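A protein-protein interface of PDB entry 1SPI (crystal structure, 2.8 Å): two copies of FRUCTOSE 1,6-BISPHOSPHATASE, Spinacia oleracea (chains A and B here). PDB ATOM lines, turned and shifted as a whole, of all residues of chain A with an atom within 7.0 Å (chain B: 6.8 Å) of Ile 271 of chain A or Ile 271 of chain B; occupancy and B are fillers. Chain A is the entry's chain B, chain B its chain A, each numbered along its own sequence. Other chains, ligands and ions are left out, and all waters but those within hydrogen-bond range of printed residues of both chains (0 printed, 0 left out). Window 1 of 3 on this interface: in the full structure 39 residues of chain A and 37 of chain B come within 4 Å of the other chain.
N of Ile 271 of chain A is in hydrogen-bond range of OD1 of Asp 277 of chain A, at 3.1 Å. The backbone carbonyl oxygen of Ser 141 of chain B lies close to the side-chain hydroxyl of Ser 273 of chain B (3.4 Å). The side-chain amide nitrogen of Asn 135 of chain A lies close to the backbone carbonyl oxygen of Gly 272 of chain A (3.3 Å). The side-chain hydroxyl (OG) of Ser 194 of chain B sits at hydrogen-bond distance from the backbone carbonyl oxygen (O) of Val 140 of chain B (2.7 Å). OD1 of Asn 135 of chain B sits close to O of Ser 141 of chain B (3.0 Å). O of Arg 269 of chain A sits at hydrogen-bond distance from OG of Ser 236 of chain A.
Among the printed residues, merely in contact across the chains: Val 140 of chain A with Ser 141 of chain B (3.1 Å), Arg 269 of chain A with Tyr 270 of chain B (3.3 Å), Ser 268 of chain A with Tyr 270 of chain B (3.4 Å), Tyr 270 of chain A with Ser 268 of chain B (3.4 Å), Tyr 270 of chain A with Arg 269 of chain B (3.4 Å), Ser 141 of chain A with Val 140 of chain B (3.5 Å), Ile 271 of chain A with Ile 271 of chain B (3.6 Å), Tyr 270 of chain A with Ile 271 of chain B (3.6 Å), Arg 280 of chain A with Ala 138 of chain B (3.6 Å), Ile 271 of chain A with Val 140 of chain B (3.7 Å), Val 140 of chain A with Val 140 of chain B (3.8 Å), Ile 271 of chain A with Tyr 270 of chain B (3.9 Å), Gly 272 of chain A with Arg 269 of chain B (3.95 Å) and Arg 280 of chain A with Val 140 of chain B (3.996 Å).
Ile 271 of chain A touches just these residues of chain B: Val 140, Tyr 270, Ile 271 and Arg 280. Of chain A, only Tyr 270, Ile 271 and Arg 280 come within 4 Å of Ile 271 of chain B. Printed residues of chain B within 4 Å of Asn 135 of chain A: Arg 280 (2.8 Å). Of the printed residues of chain A, Val 140 of chain B touches Val 140, Ser 141, Ile 271 and Arg 280. Printed residues of chain B within 4 Å of Ser 141 of chain A: Val 140. Gly 272 of chain B touches none of the printed residues of chain A. Asp 277 of chain A touches none of the printed residues of chain B. The nearest residue of chain B that does not touch Ile 271 of chain A is Arg 269 of chain B (4.2 Å). The nearest residue of chain A that does not touch Ile 271 of chain B is Arg 269 of chain A (4.1 Å).
The side-chain amide nitrogen of Asn 135 of chain A lies close to the guanidinium group of Arg 280 of chain B. The backbone carbonyl oxygen (O) of Ile 271 of chain A is in hydrogen-bond range of the guanidinium group (NH2) of Arg 280 of chain B, at 2.5 Å. NH2 of Arg 280 of chain A sits at hydrogen-bond distance from O of Ile 271 of chain B, 2.5 Å away. The backbone carbonyl oxygen (O) of Val 140 of chain A sits at hydrogen-bond distance from the side-chain hydroxyl (OG) of Ser 194 of chain B. N of Tyr 270 of chain A sits at hydrogen-bond distance from O of Tyr 270 of chain B (2.6 Å).
Ser 268 of chain A touches Tyr 270 of chain B, and with the chains exchanged Tyr 270 of chain A touches Ser 268 of chain B. Ile 271 of chain B touches its own counterpart, Ile 271 of chain A. Gly 272 of chain A touches Arg 269 of chain B, but with the chains exchanged Arg 269 of chain A does not touch Gly 272 of chain B (4.4 Å). Arg 280 of chain A touches Val 140 of chain B, but with the chains exchanged Val 140 of chain A does not touch Arg 280 of chain B (4.2 Å). Positions printed for both chains: 135, 140, 141, 236, 268, 269, 270, 271, 272, 273, 274, 276, 277, 280 and 288. Of the 19 pairs that touch across the chains among the printed residues, 13 have their exchanged pair printed and touching as well.
Hydrophobic or aromatic side chains of chain A that line the printed part of chain B: Val 140, Tyr 270 and Ile 271. Of the 18 printed residues of chain B, 9 touch a printed residue of chain A. Printed residues of chain B that touch a printed residue of chain A: Ala 138, Val 140, Ser 141, Ser 194, Ser 268, Arg 269, Tyr 270, Ile 271 and Arg 280.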
ATOM      1  N   ASN A 135       4.075  31.226 -25.109  1.00  0.00           N
ATOM      2  CA  ASN A 135       3.955  29.782 -24.949  1.00  0.00           C
ATOM      3  C   ASN A 135       2.836  29.446 -23.966  1.00  0.00           C
ATOM      4  O   ASN A 135       2.931  28.420 -23.256  1.00  0.00           O
ATOM      5  CB  ASN A 135       5.264  29.158 -24.465  1.00  0.00           C
ATOM      6  CG  ASN A 135       5.933  29.987 -23.403  1.00  0.00           C
ATOM      7  OD1 ASN A 135       5.300  30.848 -22.796  1.00  0.00           O
ATOM      8  ND2 ASN A 135       7.244  29.846 -23.266  1.00  0.00           N
ATOM      9  N   VAL A 140       1.942  25.627 -20.526  1.00  0.00           N
ATOM     10  CA  VAL A 140       2.777  24.882 -19.592  1.00  0.00           C
ATOM     11  C   VAL A 140       2.839  25.649 -18.293  1.00  0.00           C
ATOM     12  O   VAL A 140       2.550  25.059 -17.239  1.00  0.00           O
ATOM     13  CB  VAL A 140       4.219  24.525 -20.137  1.00  0.00           C
ATOM     14  CG1 VAL A 140       5.180  24.244 -19.023  1.00  0.00           C
ATOM     15  CG2 VAL A 140       4.133  23.290 -20.987  1.00  0.00           C
ATOM     16  N   SER A 141       3.107  26.961 -18.366  1.00  0.00           N
ATOM     17  CA  SER A 141       3.204  27.797 -17.159  1.00  0.00           C
ATOM     18  C   SER A 141       2.918  29.259 -17.468  1.00  0.00           C
ATOM     19  O   SER A 141       2.836  29.612 -18.625  1.00  0.00           O
ATOM     20  CB  SER A 141       4.588  27.650 -16.567  1.00  0.00           C
ATOM     21  OG  SER A 141       4.717  28.418 -15.416  1.00  0.00           O
ATOM     22  N   THR A 142       2.729  30.088 -16.438  1.00  0.00           N
ATOM     23  CA  THR A 142       2.422  31.527 -16.582  1.00  0.00           C
ATOM     24  C   THR A 142       2.428  32.118 -15.189  1.00  0.00           C
ATOM     25  O   THR A 142       2.788  31.406 -14.245  1.00  0.00           O
ATOM     26  CB  THR A 142       1.041  31.794 -17.195  1.00  0.00           C
ATOM     27  OG1 THR A 142       0.873  31.017 -18.378  1.00  0.00           O
ATOM     28  CG2 THR A 142       0.893  33.222 -17.597  1.00  0.00           C
ATOM     29  N   SER A 236      19.496  29.727 -16.159  1.00  0.00           N
ATOM     30  CA  SER A 236      18.414  29.835 -17.111  1.00  0.00           C
ATOM     31  C   SER A 236      18.601  31.118 -17.907  1.00  0.00           C
ATOM     32  O   SER A 236      18.291  32.197 -17.414  1.00  0.00           O
ATOM     33  CB  SER A 236      17.056  29.875 -16.367  1.00  0.00           C
ATOM     34  OG  SER A 236      16.942  28.913 -15.309  1.00  0.00           O
ATOM     35  N   SER A 268      21.259  23.142 -16.292  1.00  0.00           N
ATOM     36  CA  SER A 268      20.479  24.293 -16.807  1.00  0.00           C
ATOM     37  C   SER A 268      19.058  24.023 -17.183  1.00  0.00           C
ATOM     38  O   SER A 268      18.755  22.936 -17.656  1.00  0.00           O
ATOM     39  CB  SER A 268      21.055  24.801 -18.106  1.00  0.00           C
ATOM     40  OG  SER A 268      20.146  24.663 -19.207  1.00  0.00           O
ATOM     41  N   ARG A 269      18.250  25.086 -17.197  1.00  0.00           N
ATOM     42  CA  ARG A 269      16.844  24.966 -17.583  1.00  0.00           C
ATOM     43  C   ARG A 269      16.035  26.244 -17.819  1.00  0.00           C
ATOM     44  O   ARG A 269      15.908  27.099 -16.947  1.00  0.00           O
ATOM     45  CB  ARG A 269      16.113  24.055 -16.619  1.00  0.00           C
ATOM     46  CG  ARG A 269      16.482  24.209 -15.165  1.00  0.00           C
ATOM     47  CD  ARG A 269      15.850  23.058 -14.465  1.00  0.00           C
ATOM     48  NE  ARG A 269      16.005  21.885 -15.309  1.00  0.00           N
ATOM     49  CZ  ARG A 269      16.714  20.842 -14.959  1.00  0.00           C
ATOM     50  NH1 ARG A 269      17.296  20.864 -13.781  1.00  0.00           N
ATOM     51  NH2 ARG A 269      16.848  19.804 -15.768  1.00  0.00           N
ATOM     52  N   TYR A 270      15.489  26.358 -19.016  1.00  0.00           N
ATOM     53  CA  TYR A 270      14.719  27.514 -19.407  1.00  0.00           C
ATOM     54  C   TYR A 270      13.290  27.002 -19.750  1.00  0.00           C
ATOM     55  O   TYR A 270      13.143  26.164 -20.637  1.00  0.00           O
ATOM     56  CB  TYR A 270      15.447  28.165 -20.606  1.00  0.00           C
ATOM     57  CG  TYR A 270      14.974  29.552 -21.019  1.00  0.00           C
ATOM     58  CD1 TYR A 270      15.180  30.661 -20.210  1.00  0.00           C
ATOM     59  CD2 TYR A 270      14.290  29.745 -22.211  1.00  0.00           C
ATOM     60  CE1 TYR A 270      14.707  31.922 -20.584  1.00  0.00           C
ATOM     61  CE2 TYR A 270      13.817  30.994 -22.576  1.00  0.00           C
ATOM     62  CZ  TYR A 270      14.028  32.067 -21.765  1.00  0.00           C
ATOM     63  OH  TYR A 270      13.569  33.302 -22.146  1.00  0.00           O
ATOM     64  N   ILE A 271      12.272  27.429 -18.988  1.00  0.00           N
ATOM     65  CA  ILE A 271      10.884  27.004 -19.246  1.00  0.00           C
ATOM     66  C   ILE A 271      10.243  27.819 -20.346  1.00  0.00           C
ATOM     67  O   ILE A 271       9.704  27.270 -21.303  1.00  0.00           O
ATOM     68  CB  ILE A 271       9.965  27.079 -17.975  1.00  0.00           C
ATOM     69  CG1 ILE A 271      10.413  26.065 -16.917  1.00  0.00           C
ATOM     70  CG2 ILE A 271       8.533  26.791 -18.333  1.00  0.00           C
ATOM     71  CD1 ILE A 271       9.696  26.127 -15.586  1.00  0.00           C
ATOM     72  N   GLY A 272      10.299  29.139 -20.189  1.00  0.00           N
ATOM     73  CA  GLY A 272       9.704  30.054 -21.151  1.00  0.00           C
ATOM     74  C   GLY A 272       8.954  31.213 -20.507  1.00  0.00           C
ATOM     75  O   GLY A 272       8.489  32.107 -21.206  1.00  0.00           O
ATOM     76  N   SER A 273       8.814  31.203 -19.190  1.00  0.00           N
ATOM     77  CA  SER A 273       8.099  32.253 -18.503  1.00  0.00           C
ATOM     78  C   SER A 273       8.864  32.590 -17.256  1.00  0.00           C
ATOM     79  O   SER A 273       9.223  31.700 -16.507  1.00  0.00           O
ATOM     80  CB  SER A 273       6.673  31.749 -18.143  1.00  0.00           C
ATOM     81  OG  SER A 273       5.852  32.707 -17.444  1.00  0.00           O
ATOM     82  N   LEU A 274       9.030  33.885 -16.996  1.00  0.00           N
ATOM     83  CA  LEU A 274       9.743  34.377 -15.823  1.00  0.00           C
ATOM     84  C   LEU A 274       9.356  33.598 -14.584  1.00  0.00           C
ATOM     85  O   LEU A 274      10.124  32.763 -14.113  1.00  0.00           O
ATOM     86  CB  LEU A 274       9.419  35.835 -15.583  1.00  0.00           C
ATOM     87  CG  LEU A 274      10.539  36.844 -15.635  1.00  0.00           C
ATOM     88  CD1 LEU A 274       9.953  38.195 -15.326  1.00  0.00           C
ATOM     89  CD2 LEU A 274      11.639  36.499 -14.658  1.00  0.00           C
ATOM     90  N   VAL A 275       8.113  33.786 -14.145  1.00  0.00           N
ATOM     91  CA  VAL A 275       7.580  33.144 -12.948  1.00  0.00           C
ATOM     92  C   VAL A 275       7.856  31.681 -12.795  1.00  0.00           C
ATOM     93  O   VAL A 275       8.014  31.222 -11.693  1.00  0.00           O
ATOM     94  CB  VAL A 275       6.081  33.411 -12.802  1.00  0.00           C
ATOM     95  CG1 VAL A 275       5.541  32.755 -11.517  1.00  0.00           C
ATOM     96  CG2 VAL A 275       5.846  34.938 -12.770  1.00  0.00           C
ATOM     97  N   GLY A 276       7.817  30.926 -13.874  1.00  0.00           N
ATOM     98  CA  GLY A 276       8.181  29.527 -13.760  1.00  0.00           C
ATOM     99  C   GLY A 276       9.683  29.447 -13.429  1.00  0.00           C
ATOM    100  O   GLY A 276      10.063  28.815 -12.430  1.00  0.00           O
ATOM    101  N   ASP A 277      10.533  30.112 -14.228  1.00  0.00           N
ATOM    102  CA  ASP A 277      11.972  30.141 -13.998  1.00  0.00           C
ATOM    103  C   ASP A 277      12.259  30.732 -12.620  1.00  0.00           C
ATOM    104  O   ASP A 277      12.825  30.051 -11.774  1.00  0.00           O
ATOM    105  CB  ASP A 277      12.696  30.962 -15.048  1.00  0.00           C
ATOM    106  CG  ASP A 277      12.730  30.317 -16.395  1.00  0.00           C
ATOM    107  OD1 ASP A 277      13.133  29.176 -16.516  1.00  0.00           O
ATOM    108  OD2 ASP A 277      12.414  30.977 -17.378  1.00  0.00           O
ATOM    109  N   ARG A 280      11.229  28.343 -10.051  1.00  0.00           N
ATOM    110  CA  ARG A 280      12.190  27.264 -10.051  1.00  0.00           C
ATOM    111  C   ARG A 280      13.572  27.706  -9.542  1.00  0.00           C
ATOM    112  O   ARG A 280      14.331  26.901  -9.051  1.00  0.00           O
ATOM    113  CB  ARG A 280      12.251  26.616 -11.430  1.00  0.00           C
ATOM    114  CG  ARG A 280      12.831  25.226 -11.390  1.00  0.00           C
ATOM    115  CD  ARG A 280      13.922  25.039 -12.447  1.00  0.00           C
ATOM    116  NE  ARG A 280      13.462  24.871 -13.834  1.00  0.00           N
ATOM    117  CZ  ARG A 280      12.266  24.398 -14.220  1.00  0.00           C
ATOM    118  NH1 ARG A 280      11.341  24.034 -13.349  1.00  0.00           N
ATOM    119  NH2 ARG A 280      12.012  24.194 -15.505  1.00  0.00           N
ATOM    120  N   TYR A 288      19.619  33.650 -13.193  1.00  0.00           N
ATOM    121  CA  TYR A 288      18.609  33.728 -14.231  1.00  0.00           C
ATOM    122  C   TYR A 288      18.728  35.134 -14.693  1.00  0.00           C
ATOM    123  O   TYR A 288      19.034  36.013 -13.873  1.00  0.00           O
ATOM    124  CB  TYR A 288      17.206  33.546 -13.651  1.00  0.00           C
ATOM    125  CG  TYR A 288      16.125  33.900 -14.635  1.00  0.00           C
ATOM    126  CD1 TYR A 288      15.656  32.971 -15.500  1.00  0.00           C
ATOM    127  CD2 TYR A 288      15.649  35.182 -14.760  1.00  0.00           C
ATOM    128  CE1 TYR A 288      14.769  33.286 -16.457  1.00  0.00           C
ATOM    129  CE2 TYR A 288      14.760  35.501 -15.730  1.00  0.00           C
ATOM    130  CZ  TYR A 288      14.330  34.541 -16.585  1.00  0.00           C
ATOM    131  OH  TYR A 288      13.515  34.783 -17.664  1.00  0.00           O
ATOM    132  N   ASN B 135      12.161  15.438 -11.624  1.00  0.00           N
ATOM    133  CA  ASN B 135      11.198  16.257 -12.366  1.00  0.00           C
ATOM    134  C   ASN B 135      10.147  16.922 -11.514  1.00  0.00           C
ATOM    135  O   ASN B 135       9.915  18.156 -11.646  1.00  0.00           O
ATOM    136  CB  ASN B 135      10.467  15.452 -13.468  1.00  0.00           C
ATOM    137  CG  ASN B 135       9.697  16.369 -14.461  1.00  0.00           C
ATOM    138  OD1 ASN B 135       8.725  15.945 -15.105  1.00  0.00           O
ATOM    139  ND2 ASN B 135      10.170  17.608 -14.626  1.00  0.00           N
ATOM    140  N   ALA B 138      10.514  20.268  -7.953  1.00  0.00           N
ATOM    141  CA  ALA B 138      10.169  21.677  -8.147  1.00  0.00           C
ATOM    142  C   ALA B 138       9.607  21.805  -9.543  1.00  0.00           C
ATOM    143  O   ALA B 138       9.878  22.784 -10.259  1.00  0.00           O
ATOM    144  CB  ALA B 138      11.412  22.593  -7.960  1.00  0.00           C
ATOM    145  N   ALA B 139       8.811  20.803  -9.911  1.00  0.00           N
ATOM    146  CA  ALA B 139       8.191  20.729 -11.230  1.00  0.00           C
ATOM    147  C   ALA B 139       7.402  21.984 -11.656  1.00  0.00           C
ATOM    148  O   ALA B 139       7.321  22.994 -10.953  1.00  0.00           O
ATOM    149  CB  ALA B 139       7.294  19.459 -11.327  1.00  0.00           C
ATOM    150  N   VAL B 140       6.808  21.859 -12.835  1.00  0.00           N
ATOM    151  CA  VAL B 140       5.998  22.841 -13.522  1.00  0.00           C
ATOM    152  C   VAL B 140       5.336  21.985 -14.637  1.00  0.00           C
ATOM    153  O   VAL B 140       4.477  22.448 -15.357  1.00  0.00           O
ATOM    154  CB  VAL B 140       6.910  23.973 -14.109  1.00  0.00           C
ATOM    155  CG1 VAL B 140       6.152  24.899 -15.018  1.00  0.00           C
ATOM    156  CG2 VAL B 140       7.437  24.814 -13.003  1.00  0.00           C
ATOM    157  N   SER B 141       5.767  20.740 -14.798  1.00  0.00           N
ATOM    158  CA  SER B 141       5.192  19.862 -15.797  1.00  0.00           C
ATOM    159  C   SER B 141       5.571  18.431 -15.493  1.00  0.00           C
ATOM    160  O   SER B 141       6.663  18.175 -14.982  1.00  0.00           O
ATOM    161  CB  SER B 141       5.690  20.199 -17.182  1.00  0.00           C
ATOM    162  OG  SER B 141       5.313  21.499 -17.540  1.00  0.00           O
ATOM    163  N   SER B 194       0.169  19.918 -16.422  1.00  0.00           N
ATOM    164  CA  SER B 194       0.842  21.200 -16.375  1.00  0.00           C
ATOM    165  C   SER B 194       0.022  22.340 -16.991  1.00  0.00           C
ATOM    166  O   SER B 194      -0.220  22.322 -18.210  1.00  0.00           O
ATOM    167  CB  SER B 194       2.179  21.067 -17.113  1.00  0.00           C
ATOM    168  OG  SER B 194       2.787  22.321 -17.434  1.00  0.00           O
ATOM    169  N   SER B 236      15.859  21.787 -27.758  1.00  0.00           N
ATOM    170  CA  SER B 236      15.744  21.402 -26.357  1.00  0.00           C
ATOM    171  C   SER B 236      16.774  20.338 -26.051  1.00  0.00           C
ATOM    172  O   SER B 236      16.592  19.170 -26.428  1.00  0.00           O
ATOM    173  CB  SER B 236      14.326  20.849 -26.108  1.00  0.00           C
ATOM    174  OG  SER B 236      13.321  21.739 -26.628  1.00  0.00           O
ATOM    175  N   SER B 268      16.562  28.167 -27.397  1.00  0.00           N
ATOM    176  CA  SER B 268      16.520  26.905 -26.661  1.00  0.00           C
ATOM    177  C   SER B 268      15.481  26.922 -25.540  1.00  0.00           C
ATOM    178  O   SER B 268      15.301  27.943 -24.872  1.00  0.00           O
ATOM    179  CB  SER B 268      17.866  26.611 -26.022  1.00  0.00           C
ATOM    180  OG  SER B 268      18.134  27.625 -25.079  1.00  0.00           O
ATOM    181  N   ARG B 269      14.805  25.792 -25.333  1.00  0.00           N
ATOM    182  CA  ARG B 269      13.842  25.657 -24.255  1.00  0.00           C
ATOM    183  C   ARG B 269      14.103  24.258 -23.694  1.00  0.00           C
ATOM    184  O   ARG B 269      14.266  23.288 -24.444  1.00  0.00           O
ATOM    185  CB  ARG B 269      12.391  25.786 -24.732  1.00  0.00           C
ATOM    186  CG  ARG B 269      11.985  27.080 -25.393  1.00  0.00           C
ATOM    187  CD  ARG B 269      12.173  28.302 -24.511  1.00  0.00           C
ATOM    188  NE  ARG B 269      11.184  29.368 -24.750  1.00  0.00           N
ATOM    189  CZ  ARG B 269      11.071  30.074 -25.864  1.00  0.00           C
ATOM    190  NH1 ARG B 269      11.884  29.860 -26.875  1.00  0.00           N
ATOM    191  NH2 ARG B 269      10.128  30.982 -25.985  1.00  0.00           N
ATOM    192  N   TYR B 270      14.286  24.206 -22.386  1.00  0.00           N
ATOM    193  CA  TYR B 270      14.498  22.972 -21.661  1.00  0.00           C
ATOM    194  C   TYR B 270      13.761  23.257 -20.330  1.00  0.00           C
ATOM    195  O   TYR B 270      14.208  24.091 -19.507  1.00  0.00           O
ATOM    196  CB  TYR B 270      15.987  22.719 -21.440  1.00  0.00           C
ATOM    197  CG  TYR B 270      16.303  21.330 -20.946  1.00  0.00           C
ATOM    198  CD1 TYR B 270      16.080  20.235 -21.730  1.00  0.00           C
ATOM    199  CD2 TYR B 270      16.767  21.117 -19.671  1.00  0.00           C
ATOM    200  CE1 TYR B 270      16.296  18.965 -21.260  1.00  0.00           C
ATOM    201  CE2 TYR B 270      16.988  19.845 -19.193  1.00  0.00           C
ATOM    202  CZ  TYR B 270      16.743  18.777 -19.992  1.00  0.00           C
ATOM    203  OH  TYR B 270      16.913  17.505 -19.506  1.00  0.00           O
ATOM    204  N   ILE B 271      12.562  22.668 -20.196  1.00  0.00           N
ATOM    205  CA  ILE B 271      11.698  22.838 -19.016  1.00  0.00           C
ATOM    206  C   ILE B 271      12.146  21.833 -18.014  1.00  0.00           C
ATOM    207  O   ILE B 271      12.204  22.113 -16.833  1.00  0.00           O
ATOM    208  CB  ILE B 271      10.206  22.572 -19.398  1.00  0.00           C
ATOM    209  CG1 ILE B 271       9.593  23.792 -20.066  1.00  0.00           C
ATOM    210  CG2 ILE B 271       9.386  22.120 -18.243  1.00  0.00           C
ATOM    211  CD1 ILE B 271       8.977  23.439 -21.321  1.00  0.00           C
ATOM    212  N   GLY B 272      12.502  20.667 -18.534  1.00  0.00           N
ATOM    213  CA  GLY B 272      12.925  19.568 -17.707  1.00  0.00           C
ATOM    214  C   GLY B 272      12.049  18.393 -18.100  1.00  0.00           C
ATOM    215  O   GLY B 272      12.481  17.534 -18.887  1.00  0.00           O
ATOM    216  N   SER B 273      10.800  18.395 -17.626  1.00  0.00           N
ATOM    217  CA  SER B 273       9.847  17.331 -17.915  1.00  0.00           C
ATOM    218  C   SER B 273       9.764  16.911 -19.370  1.00  0.00           C
ATOM    219  O   SER B 273       9.606  17.732 -20.258  1.00  0.00           O
ATOM    220  CB  SER B 273       8.439  17.698 -17.419  1.00  0.00           C
ATOM    221  OG  SER B 273       7.842  18.770 -18.168  1.00  0.00           O
ATOM    222  N   LEU B 274       9.778  15.592 -19.555  1.00  0.00           N
ATOM    223  CA  LEU B 274       9.723  14.911 -20.846  1.00  0.00           C
ATOM    224  C   LEU B 274       8.443  15.173 -21.598  1.00  0.00           C
ATOM    225  O   LEU B 274       8.454  15.315 -22.813  1.00  0.00           O
ATOM    226  CB  LEU B 274       9.911  13.430 -20.621  1.00  0.00           C
ATOM    227  CG  LEU B 274       9.423  12.434 -21.637  1.00  0.00           C
ATOM    228  CD1 LEU B 274      10.016  12.682 -22.995  1.00  0.00           C
ATOM    229  CD2 LEU B 274       9.758  11.037 -21.108  1.00  0.00           C
ATOM    230  N   GLY B 276       6.372  17.799 -20.708  1.00  0.00           N
ATOM    231  CA  GLY B 276       6.375  19.243 -20.785  1.00  0.00           C
ATOM    232  C   GLY B 276       7.086  19.625 -22.044  1.00  0.00           C
ATOM    233  O   GLY B 276       6.510  20.317 -22.880  1.00  0.00           O
ATOM    234  N   ASP B 277       8.291  19.066 -22.214  1.00  0.00           N
ATOM    235  CA  ASP B 277       9.136  19.292 -23.389  1.00  0.00           C
ATOM    236  C   ASP B 277       8.590  18.613 -24.613  1.00  0.00           C
ATOM    237  O   ASP B 277       8.559  19.234 -25.667  1.00  0.00           O
ATOM    238  CB  ASP B 277      10.569  18.831 -23.164  1.00  0.00           C
ATOM    239  CG  ASP B 277      11.353  19.760 -22.257  1.00  0.00           C
ATOM    240  OD1 ASP B 277      11.235  20.999 -22.404  1.00  0.00           O
ATOM    241  OD2 ASP B 277      12.086  19.248 -21.394  1.00  0.00           O
ATOM    242  N   ARG B 280       5.679  20.853 -25.936  1.00  0.00           N
ATOM    243  CA  ARG B 280       6.053  22.140 -26.504  1.00  0.00           C
ATOM    244  C   ARG B 280       6.476  21.895 -27.924  1.00  0.00           C
ATOM    245  O   ARG B 280       5.987  22.542 -28.834  1.00  0.00           O
ATOM    246  CB  ARG B 280       7.203  22.754 -25.741  1.00  0.00           C
ATOM    247  CG  ARG B 280       7.479  24.195 -26.153  1.00  0.00           C
ATOM    248  CD  ARG B 280       8.600  24.782 -25.300  1.00  0.00           C
ATOM    249  NE  ARG B 280       8.234  24.892 -23.882  1.00  0.00           N
ATOM    250  CZ  ARG B 280       7.932  26.043 -23.271  1.00  0.00           C
ATOM    251  NH1 ARG B 280       7.939  27.178 -23.949  1.00  0.00           N
ATOM    252  NH2 ARG B 280       7.665  26.077 -21.977  1.00  0.00           N
ATOM    253  N   TYR B 288      13.749  18.105 -29.465  1.00  0.00           N
ATOM    254  CA  TYR B 288      14.083  17.847 -28.064  1.00  0.00           C
ATOM    255  C   TYR B 288      14.970  16.645 -28.236  1.00  0.00           C
ATOM    256  O   TYR B 288      14.854  15.950 -29.239  1.00  0.00           O
ATOM    257  CB  TYR B 288      12.826  17.429 -27.264  1.00  0.00           C
ATOM    258  CG  TYR B 288      13.075  16.766 -25.907  1.00  0.00           C
ATOM    259  CD1 TYR B 288      13.352  17.496 -24.782  1.00  0.00           C
ATOM    260  CD2 TYR B 288      12.978  15.426 -25.755  1.00  0.00           C
ATOM    261  CE1 TYR B 288      13.524  16.888 -23.547  1.00  0.00           C
ATOM    262  CE2 TYR B 288      13.141  14.821 -24.526  1.00  0.00           C
ATOM    263  CZ  TYR B 288      13.410  15.550 -23.440  1.00  0.00           C
ATOM    264  OH  TYR B 288      13.560  14.912 -22.240  1.00  0.00           O
